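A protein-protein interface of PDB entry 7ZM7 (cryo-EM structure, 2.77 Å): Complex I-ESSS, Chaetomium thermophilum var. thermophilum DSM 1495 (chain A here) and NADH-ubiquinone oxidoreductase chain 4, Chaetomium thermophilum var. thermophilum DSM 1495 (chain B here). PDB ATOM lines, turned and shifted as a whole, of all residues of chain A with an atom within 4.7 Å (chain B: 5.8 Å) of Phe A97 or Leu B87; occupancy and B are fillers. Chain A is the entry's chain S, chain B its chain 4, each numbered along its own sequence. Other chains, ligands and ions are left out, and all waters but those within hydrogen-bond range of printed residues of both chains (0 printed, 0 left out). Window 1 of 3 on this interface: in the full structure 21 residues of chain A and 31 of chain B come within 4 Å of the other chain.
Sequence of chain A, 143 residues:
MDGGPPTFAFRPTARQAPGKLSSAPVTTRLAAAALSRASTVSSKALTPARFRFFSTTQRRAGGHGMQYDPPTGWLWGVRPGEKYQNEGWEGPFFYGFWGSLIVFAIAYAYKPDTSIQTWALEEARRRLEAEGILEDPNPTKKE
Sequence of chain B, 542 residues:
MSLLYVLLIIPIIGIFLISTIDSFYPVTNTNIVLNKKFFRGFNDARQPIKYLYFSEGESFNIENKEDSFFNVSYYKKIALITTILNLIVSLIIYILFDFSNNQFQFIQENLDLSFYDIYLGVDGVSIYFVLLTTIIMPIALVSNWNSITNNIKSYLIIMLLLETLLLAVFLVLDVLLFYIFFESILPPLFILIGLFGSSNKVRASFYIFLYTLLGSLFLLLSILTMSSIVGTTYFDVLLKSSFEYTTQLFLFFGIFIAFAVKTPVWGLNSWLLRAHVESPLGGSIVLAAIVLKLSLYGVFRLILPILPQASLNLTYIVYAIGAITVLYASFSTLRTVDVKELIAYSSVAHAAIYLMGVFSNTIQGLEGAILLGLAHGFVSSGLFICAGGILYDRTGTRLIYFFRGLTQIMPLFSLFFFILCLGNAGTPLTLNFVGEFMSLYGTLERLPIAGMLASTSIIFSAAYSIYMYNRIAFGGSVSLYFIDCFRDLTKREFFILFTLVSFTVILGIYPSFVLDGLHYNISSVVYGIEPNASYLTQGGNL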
ATOM      1  N   PRO A  92      19.045 -34.858  -6.519  1.00  0.00           N
ATOM      2  CA  PRO A  92      19.539 -33.481  -6.644  1.00  0.00           C
ATOM      3  C   PRO A  92      19.988 -32.860  -5.333  1.00  0.00           C
ATOM      4  O   PRO A  92      20.855 -31.982  -5.350  1.00  0.00           O
ATOM      5  CB  PRO A  92      18.338 -32.732  -7.233  1.00  0.00           C
ATOM      6  CG  PRO A  92      17.386 -33.790  -7.678  1.00  0.00           C
ATOM      7  CD  PRO A  92      17.606 -34.943  -6.800  1.00  0.00           C
ATOM      8  N   PHE A  93      19.426 -33.276  -4.200  1.00  0.00           N
ATOM      9  CA  PHE A  93      19.752 -32.623  -2.938  1.00  0.00           C
ATOM     10  C   PHE A  93      21.174 -32.928  -2.503  1.00  0.00           C
ATOM     11  O   PHE A  93      21.806 -32.116  -1.827  1.00  0.00           O
ATOM     12  CB  PHE A  93      18.743 -33.046  -1.876  1.00  0.00           C
ATOM     13  CG  PHE A  93      18.932 -32.387  -0.540  1.00  0.00           C
ATOM     14  CD1 PHE A  93      19.855 -32.853   0.375  1.00  0.00           C
ATOM     15  CD2 PHE A  93      18.180 -31.283  -0.203  1.00  0.00           C
ATOM     16  CE1 PHE A  93      20.018 -32.234   1.582  1.00  0.00           C
ATOM     17  CE2 PHE A  93      18.344 -30.672   1.001  1.00  0.00           C
ATOM     18  CZ  PHE A  93      19.261 -31.157   1.895  1.00  0.00           C
ATOM     19  N   TYR A  95      23.793 -34.069  -4.691  1.00  0.00           N
ATOM     20  CA  TYR A  95      24.754 -33.679  -5.705  1.00  0.00           C
ATOM     21  C   TYR A  95      24.661 -32.202  -6.037  1.00  0.00           C
ATOM     22  O   TYR A  95      25.687 -31.527  -6.146  1.00  0.00           O
ATOM     23  CB  TYR A  95      24.536 -34.493  -6.974  1.00  0.00           C
ATOM     24  CG  TYR A  95      24.850 -35.948  -6.821  1.00  0.00           C
ATOM     25  CD1 TYR A  95      26.009 -36.361  -6.185  1.00  0.00           C
ATOM     26  CD2 TYR A  95      23.997 -36.913  -7.323  1.00  0.00           C
ATOM     27  CE1 TYR A  95      26.306 -37.696  -6.045  1.00  0.00           C
ATOM     28  CE2 TYR A  95      24.286 -38.252  -7.191  1.00  0.00           C
ATOM     29  CZ  TYR A  95      25.441 -38.637  -6.551  1.00  0.00           C
ATOM     30  OH  TYR A  95      25.731 -39.973  -6.415  1.00  0.00           O
ATOM     31  N   GLY A  96      23.450 -31.692  -6.199  1.00  0.00           N
ATOM     32  CA  GLY A  96      23.271 -30.320  -6.600  1.00  0.00           C
ATOM     33  C   GLY A  96      23.281 -29.373  -5.432  1.00  0.00           C
ATOM     34  O   GLY A  96      24.030 -28.400  -5.441  1.00  0.00           O
ATOM     35  N   PHE A  97      22.454 -29.638  -4.421  1.00  0.00           N
ATOM     36  CA  PHE A  97      22.338 -28.716  -3.301  1.00  0.00           C
ATOM     37  C   PHE A  97      23.638 -28.701  -2.522  1.00  0.00           C
ATOM     38  O   PHE A  97      24.316 -27.680  -2.480  1.00  0.00           O
ATOM     39  CB  PHE A  97      21.165 -29.080  -2.395  1.00  0.00           C
ATOM     40  CG  PHE A  97      20.887 -28.064  -1.329  1.00  0.00           C
ATOM     41  CD1 PHE A  97      20.107 -26.958  -1.597  1.00  0.00           C
ATOM     42  CD2 PHE A  97      21.414 -28.205  -0.062  1.00  0.00           C
ATOM     43  CE1 PHE A  97      19.850 -26.021  -0.613  1.00  0.00           C
ATOM     44  CE2 PHE A  97      21.167 -27.274   0.907  1.00  0.00           C
ATOM     45  CZ  PHE A  97      20.388 -26.182   0.631  1.00  0.00           C
ATOM     46  N   TRP A  98      24.035 -29.833  -1.957  1.00  0.00           N
ATOM     47  CA  TRP A  98      25.266 -29.841  -1.178  1.00  0.00           C
ATOM     48  C   TRP A  98      26.481 -29.639  -2.060  1.00  0.00           C
ATOM     49  O   TRP A  98      27.352 -28.835  -1.728  1.00  0.00           O
ATOM     50  CB  TRP A  98      25.389 -31.126  -0.373  1.00  0.00           C
ATOM     51  CG  TRP A  98      24.643 -31.012   0.885  1.00  0.00           C
ATOM     52  CD1 TRP A  98      23.386 -31.445   1.121  1.00  0.00           C
ATOM     53  CD2 TRP A  98      25.078 -30.368   2.083  1.00  0.00           C
ATOM     54  NE1 TRP A  98      23.012 -31.141   2.400  1.00  0.00           N
ATOM     55  CE2 TRP A  98      24.039 -30.479   3.011  1.00  0.00           C
ATOM     56  CE3 TRP A  98      26.256 -29.721   2.461  1.00  0.00           C
ATOM     57  CZ2 TRP A  98      24.136 -29.975   4.289  1.00  0.00           C
ATOM     58  CZ3 TRP A  98      26.345 -29.215   3.725  1.00  0.00           C
ATOM     59  CH2 TRP A  98      25.293 -29.345   4.627  1.00  0.00           C
ATOM     60  N   GLY A  99      26.545 -30.326  -3.201  1.00  0.00           N
ATOM     61  CA  GLY A  99      27.685 -30.157  -4.080  1.00  0.00           C
ATOM     62  C   GLY A  99      27.932 -28.714  -4.462  1.00  0.00           C
ATOM     63  O   GLY A  99      29.082 -28.292  -4.599  1.00  0.00           O
ATOM     64  N   SER A 100      26.867 -27.929  -4.605  1.00  0.00           N
ATOM     65  CA  SER A 100      27.025 -26.512  -4.896  1.00  0.00           C
ATOM     66  C   SER A 100      27.708 -25.783  -3.746  1.00  0.00           C
ATOM     67  O   SER A 100      28.495 -24.861  -3.971  1.00  0.00           O
ATOM     68  CB  SER A 100      25.665 -25.889  -5.204  1.00  0.00           C
ATOM     69  OG  SER A 100      25.782 -24.504  -5.465  1.00  0.00           O
ATOM     70  N   LEU A 101      27.419 -26.186  -2.510  1.00  0.00           N
ATOM     71  CA  LEU A 101      28.045 -25.557  -1.350  1.00  0.00           C
ATOM     72  C   LEU A 101      29.502 -25.957  -1.179  1.00  0.00           C
ATOM     73  O   LEU A 101      30.308 -25.139  -0.732  1.00  0.00           O
ATOM     74  CB  LEU A 101      27.251 -25.853  -0.084  1.00  0.00           C
ATOM     75  CG  LEU A 101      25.971 -25.057   0.183  1.00  0.00           C
ATOM     76  CD1 LEU A 101      24.795 -25.369  -0.703  1.00  0.00           C
ATOM     77  CD2 LEU A 101      25.593 -25.292   1.621  1.00  0.00           C
ATOM     78  N   THR B  83      15.147 -25.115  -8.428  1.00  0.00           N
ATOM     79  CA  THR B  83      15.543 -24.292  -7.290  1.00  0.00           C
ATOM     80  C   THR B  83      16.993 -24.531  -6.889  1.00  0.00           C
ATOM     81  O   THR B  83      17.597 -23.684  -6.229  1.00  0.00           O
ATOM     82  CB  THR B  83      14.614 -24.534  -6.095  1.00  0.00           C
ATOM     83  OG1 THR B  83      14.622 -25.918  -5.737  1.00  0.00           O
ATOM     84  CG2 THR B  83      13.212 -24.089  -6.382  1.00  0.00           C
ATOM     85  N   ILE B  84      17.564 -25.666  -7.277  1.00  0.00           N
ATOM     86  CA  ILE B  84      18.999 -25.874  -7.133  1.00  0.00           C
ATOM     87  C   ILE B  84      19.768 -24.926  -8.041  1.00  0.00           C
ATOM     88  O   ILE B  84      20.782 -24.350  -7.643  1.00  0.00           O
ATOM     89  CB  ILE B  84      19.351 -27.347  -7.420  1.00  0.00           C
ATOM     90  CG1 ILE B  84      18.640 -28.261  -6.430  1.00  0.00           C
ATOM     91  CG2 ILE B  84      20.835 -27.578  -7.374  1.00  0.00           C
ATOM     92  CD1 ILE B  84      18.816 -27.855  -4.997  1.00  0.00           C
ATOM     93  N   LEU B  85      19.299 -24.755  -9.273  1.00  0.00           N
ATOM     94  CA  LEU B  85      19.993 -23.896 -10.221  1.00  0.00           C
ATOM     95  C   LEU B  85      20.007 -22.444  -9.759  1.00  0.00           C
ATOM     96  O   LEU B  85      21.022 -21.757  -9.884  1.00  0.00           O
ATOM     97  CB  LEU B  85      19.344 -24.029 -11.595  1.00  0.00           C
ATOM     98  CG  LEU B  85      19.376 -25.444 -12.158  1.00  0.00           C
ATOM     99  CD1 LEU B  85      18.516 -25.555 -13.389  1.00  0.00           C
ATOM    100  CD2 LEU B  85      20.789 -25.815 -12.480  1.00  0.00           C
ATOM    101  N   ASN B  86      18.892 -21.960  -9.215  1.00  0.00           N
ATOM    102  CA  ASN B  86      18.878 -20.612  -8.663  1.00  0.00           C
ATOM    103  C   ASN B  86      19.902 -20.457  -7.557  1.00  0.00           C
ATOM    104  O   ASN B  86      20.553 -19.416  -7.444  1.00  0.00           O
ATOM    105  CB  ASN B  86      17.500 -20.277  -8.120  1.00  0.00           C
ATOM    106  CG  ASN B  86      16.641 -19.657  -9.130  1.00  0.00           C
ATOM    107  OD1 ASN B  86      17.089 -18.843  -9.920  1.00  0.00           O
ATOM    108  ND2 ASN B  86      15.386 -20.029  -9.122  1.00  0.00           N
ATOM    109  N   LEU B  87      20.026 -21.472  -6.706  1.00  0.00           N
ATOM    110  CA  LEU B  87      21.046 -21.457  -5.675  1.00  0.00           C
ATOM    111  C   LEU B  87      22.440 -21.501  -6.279  1.00  0.00           C
ATOM    112  O   LEU B  87      23.351 -20.832  -5.793  1.00  0.00           O
ATOM    113  CB  LEU B  87      20.817 -22.621  -4.721  1.00  0.00           C
ATOM    114  CG  LEU B  87      21.890 -22.798  -3.659  1.00  0.00           C
ATOM    115  CD1 LEU B  87      22.044 -21.523  -2.890  1.00  0.00           C
ATOM    116  CD2 LEU B  87      21.522 -23.926  -2.762  1.00  0.00           C
ATOM    117  N   ILE B  88      22.630 -22.281  -7.336  1.00  0.00           N
ATOM    118  CA  ILE B  88      23.931 -22.331  -8.001  1.00  0.00           C
ATOM    119  C   ILE B  88      24.293 -20.966  -8.559  1.00  0.00           C
ATOM    120  O   ILE B  88      25.396 -20.460  -8.343  1.00  0.00           O
ATOM    121  CB  ILE B  88      23.918 -23.401  -9.104  1.00  0.00           C
ATOM    122  CG1 ILE B  88      24.014 -24.795  -8.481  1.00  0.00           C
ATOM    123  CG2 ILE B  88      25.001 -23.126 -10.136  1.00  0.00           C
ATOM    124  CD1 ILE B  88      23.397 -25.873  -9.322  1.00  0.00           C
ATOM    125  N   VAL B  89      23.358 -20.343  -9.273  1.00  0.00           N
ATOM    126  CA  VAL B  89      23.597 -19.020  -9.840  1.00  0.00           C
ATOM    127  C   VAL B  89      23.854 -18.002  -8.740  1.00  0.00           C
ATOM    128  O   VAL B  89      24.747 -17.158  -8.850  1.00  0.00           O
ATOM    129  CB  VAL B  89      22.408 -18.609 -10.725  1.00  0.00           C
ATOM    130  CG1 VAL B  89      22.522 -17.161 -11.141  1.00  0.00           C
ATOM    131  CG2 VAL B  89      22.344 -19.501 -11.930  1.00  0.00           C
ATOM    132  N   SER B  90      23.078 -18.062  -7.663  1.00  0.00           N
ATOM    133  CA  SER B  90      23.176 -17.047  -6.628  1.00  0.00           C
ATOM    134  C   SER B  90      24.534 -17.079  -5.942  1.00  0.00           C
ATOM    135  O   SER B  90      25.019 -16.047  -5.470  1.00  0.00           O
ATOM    136  CB  SER B  90      22.052 -17.232  -5.622  1.00  0.00           C
ATOM    137  OG  SER B  90      22.367 -18.257  -4.708  1.00  0.00           O
ATOM    138  N   LEU B  91      25.152 -18.256  -5.850  1.00  0.00           N
ATOM    139  CA  LEU B  91      26.505 -18.346  -5.320  1.00  0.00           C
ATOM    140  C   LEU B  91      27.534 -17.869  -6.336  1.00  0.00           C
ATOM    141  O   LEU B  91      28.598 -17.379  -5.957  1.00  0.00           O
ATOM    142  CB  LEU B  91      26.797 -19.776  -4.883  1.00  0.00           C
ATOM    143  CG  LEU B  91      25.877 -20.330  -3.801  1.00  0.00           C
ATOM    144  CD1 LEU B  91      25.843 -21.847  -3.845  1.00  0.00           C
ATOM    145  CD2 LEU B  91      26.250 -19.835  -2.409  1.00  0.00           C
ATOM    146  N   ILE B  92      27.240 -18.008  -7.623  1.00  0.00           N
ATOM    147  CA  ILE B  92      28.092 -17.415  -8.647  1.00  0.00           C
ATOM    148  C   ILE B  92      28.062 -15.897  -8.543  1.00  0.00           C
ATOM    149  O   ILE B  92      29.100 -15.234  -8.643  1.00  0.00           O
ATOM    150  CB  ILE B  92      27.659 -17.909 -10.038  1.00  0.00           C
ATOM    151  CG1 ILE B  92      27.920 -19.408 -10.147  1.00  0.00           C
ATOM    152  CG2 ILE B  92      28.380 -17.157 -11.120  1.00  0.00           C
ATOM    153  CD1 ILE B  92      26.992 -20.109 -11.051  1.00  0.00           C
ATOM    154  N   LEU B 131      20.598 -14.574  -0.961  1.00  0.00           N
ATOM    155  CA  LEU B 131      21.177 -15.887  -0.710  1.00  0.00           C
ATOM    156  C   LEU B 131      20.313 -16.714   0.225  1.00  0.00           C
ATOM    157  O   LEU B 131      20.149 -17.918   0.021  1.00  0.00           O
ATOM    158  CB  LEU B 131      22.578 -15.741  -0.133  1.00  0.00           C
ATOM    159  CG  LEU B 131      23.708 -15.626  -1.144  1.00  0.00           C
ATOM    160  CD1 LEU B 131      24.846 -14.859  -0.532  1.00  0.00           C
ATOM    161  CD2 LEU B 131      24.145 -16.987  -1.568  1.00  0.00           C
ATOM    162  N   THR B 134      17.420 -18.211  -1.719  1.00  0.00           N
ATOM    163  CA  THR B 134      17.729 -19.299  -2.629  1.00  0.00           C
ATOM    164  C   THR B 134      18.197 -20.561  -1.913  1.00  0.00           C
ATOM    165  O   THR B 134      18.094 -21.648  -2.478  1.00  0.00           O
ATOM    166  CB  THR B 134      18.762 -18.825  -3.648  1.00  0.00           C
ATOM    167  OG1 THR B 134      19.937 -18.378  -2.973  1.00  0.00           O
ATOM    168  CG2 THR B 134      18.206 -17.661  -4.422  1.00  0.00           C
ATOM    169  N   ILE B 135      18.691 -20.444  -0.687  1.00  0.00           N
ATOM    170  CA  ILE B 135      19.000 -21.630   0.100  1.00  0.00           C
ATOM    171  C   ILE B 135      17.740 -22.193   0.726  1.00  0.00           C
ATOM    172  O   ILE B 135      17.590 -23.404   0.858  1.00  0.00           O
ATOM    173  CB  ILE B 135      20.055 -21.307   1.169  1.00  0.00           C
ATOM    174  CG1 ILE B 135      21.355 -20.833   0.539  1.00  0.00           C
ATOM    175  CG2 ILE B 135      20.301 -22.504   2.041  1.00  0.00           C
ATOM    176  CD1 ILE B 135      22.219 -20.082   1.500  1.00  0.00           C
ATOM    177  N   PRO B 138      14.815 -24.609  -1.677  1.00  0.00           N
ATOM    178  CA  PRO B 138      14.926 -26.062  -1.857  1.00  0.00           C
ATOM    179  C   PRO B 138      14.519 -26.869  -0.633  1.00  0.00           C
ATOM    180  O   PRO B 138      13.841 -27.886  -0.779  1.00  0.00           O
ATOM    181  CB  PRO B 138      16.405 -26.244  -2.202  1.00  0.00           C
ATOM    182  CG  PRO B 138      16.785 -25.016  -2.796  1.00  0.00           C
ATOM    183  CD  PRO B 138      16.075 -23.957  -2.049  1.00  0.00           C
ATOM    184  N   ILE B 139      14.934 -26.469   0.566  1.00  0.00           N
ATOM    185  CA  ILE B 139      14.474 -27.154   1.771  1.00  0.00           C
ATOM    186  C   ILE B 139      12.965 -27.051   1.910  1.00  0.00           C
ATOM    187  O   ILE B 139      12.306 -28.001   2.342  1.00  0.00           O
ATOM    188  CB  ILE B 139      15.195 -26.622   3.024  1.00  0.00           C
ATOM    189  CG1 ILE B 139      16.678 -26.959   2.975  1.00  0.00           C
ATOM    190  CG2 ILE B 139      14.560 -27.153   4.285  1.00  0.00           C
ATOM    191  CD1 ILE B 139      17.494 -25.970   2.335  1.00  0.00           C
ATOM    192  N   GLU B 163       9.148 -17.854  -5.424  1.00  0.00           N
ATOM    193  CA  GLU B 163      10.582 -17.627  -5.380  1.00  0.00           C
ATOM    194  C   GLU B 163      10.983 -16.515  -6.334  1.00  0.00           C
ATOM    195  O   GLU B 163      11.913 -15.756  -6.059  1.00  0.00           O
ATOM    196  CB  GLU B 163      11.339 -18.907  -5.702  1.00  0.00           C
ATOM    197  CG  GLU B 163      12.808 -18.681  -5.553  1.00  0.00           C
ATOM    198  CD  GLU B 163      13.642 -19.890  -5.794  1.00  0.00           C
ATOM    199  OE1 GLU B 163      13.069 -20.941  -6.119  1.00  0.00           O
ATOM    200  OE2 GLU B 163      14.869 -19.789  -5.585  1.00  0.00           O
ATOM    201  N   THR B 499      20.927 -29.818   7.483  1.00  0.00           N
ATOM    202  CA  THR B 499      21.372 -28.709   6.648  1.00  0.00           C
ATOM    203  C   THR B 499      21.095 -27.373   7.316  1.00  0.00           C
ATOM    204  O   THR B 499      21.975 -26.515   7.404  1.00  0.00           O
ATOM    205  CB  THR B 499      20.684 -28.775   5.291  1.00  0.00           C
ATOM    206  OG1 THR B 499      20.889 -30.068   4.725  1.00  0.00           O
ATOM    207  CG2 THR B 499      21.258 -27.737   4.369  1.00  0.00           C
ATOM    208  N   PHE B 503      23.957 -24.480   9.016  1.00  0.00           N
ATOM    209  CA  PHE B 503      24.072 -23.064   8.695  1.00  0.00           C
ATOM    210  C   PHE B 503      24.126 -22.222   9.963  1.00  0.00           C
ATOM    211  O   PHE B 503      24.871 -21.243  10.046  1.00  0.00           O
ATOM    212  CB  PHE B 503      22.890 -22.645   7.836  1.00  0.00           C
ATOM    213  CG  PHE B 503      23.116 -22.805   6.373  1.00  0.00           C
ATOM    214  CD1 PHE B 503      23.956 -21.950   5.685  1.00  0.00           C
ATOM    215  CD2 PHE B 503      22.482 -23.808   5.680  1.00  0.00           C
ATOM    216  CE1 PHE B 503      24.153 -22.100   4.330  1.00  0.00           C
ATOM    217  CE2 PHE B 503      22.681 -23.961   4.337  1.00  0.00           C
ATOM    218  CZ  PHE B 503      23.515 -23.109   3.659  1.00  0.00           C
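Among the printed residues, merely in contact across the chains: Phe A93 with Thr B499, Gly A96 with Ile B84, Phe A97 with Ile B84, Phe A97 with Leu B87, Phe A97 with Ile B135, Phe A97 with Pro B138, Phe A97 with Ile B139, Phe A97 with Thr B499, Ser A100 with Ile B88, Ser A100 with Leu B91 and Leu A101 with Phe B503.
The backbone NH (N) of Phe A97 lies within hydrogen-bond range of the backbone carbonyl oxygen (O) of Pro A92, 3.0 Å away.
O of Phe A93 is in hydrogen-bond range of N of Trp A98, at 3.2 Å.
The backbone carbonyl oxygen (O) of Leu B87 is in hydrogen-bond range of the side-chain hydroxyl (OG) of Ser B90 (3.0 Å).
Printed residues of chain B that touch a printed residue of chain A: Ile B84, Leu B87, Ile B88, Leu B91, Ile B135, Pro B138, Ile B139, Thr B499 and Phe B503.
Hydrophobic or aromatic side chains of chain A within 4 Å of the printed part of chain B: Phe A93, Phe A97, Trp A98 and Leu A101.
Among the printed residues, 12 pairs touch across the chains.
OG1 of Thr B499 sits close to NE1 of Trp A98.
Of the printed residues of chain B, Gly A96 touches Ile B84 (3.6 Å).
Of the printed residues of chain B, Phe A97 touches Ile B84 (3.7 Å), Leu B87 (3.4 Å), Ile B135 (3.8 Å), Pro B138 (3.8 Å), Ile B139 (3.4 Å) and Thr B499 (3.5 Å).
Of the printed residues of chain A, Ile B84 touches Gly A96 and Phe A97.
Leu B85 touches none of the printed residues of chain A.
Leu B131 touches none of the printed residues of chain A.
Of the printed residues of chain A, Ile B139 touches Phe A97.
The nearest residue of chain B that does not touch Phe A97 is Phe B503 (4.9 Å).
The nearest residue of chain A that does not touch Leu B87 is Leu A101 (4.1 Å).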
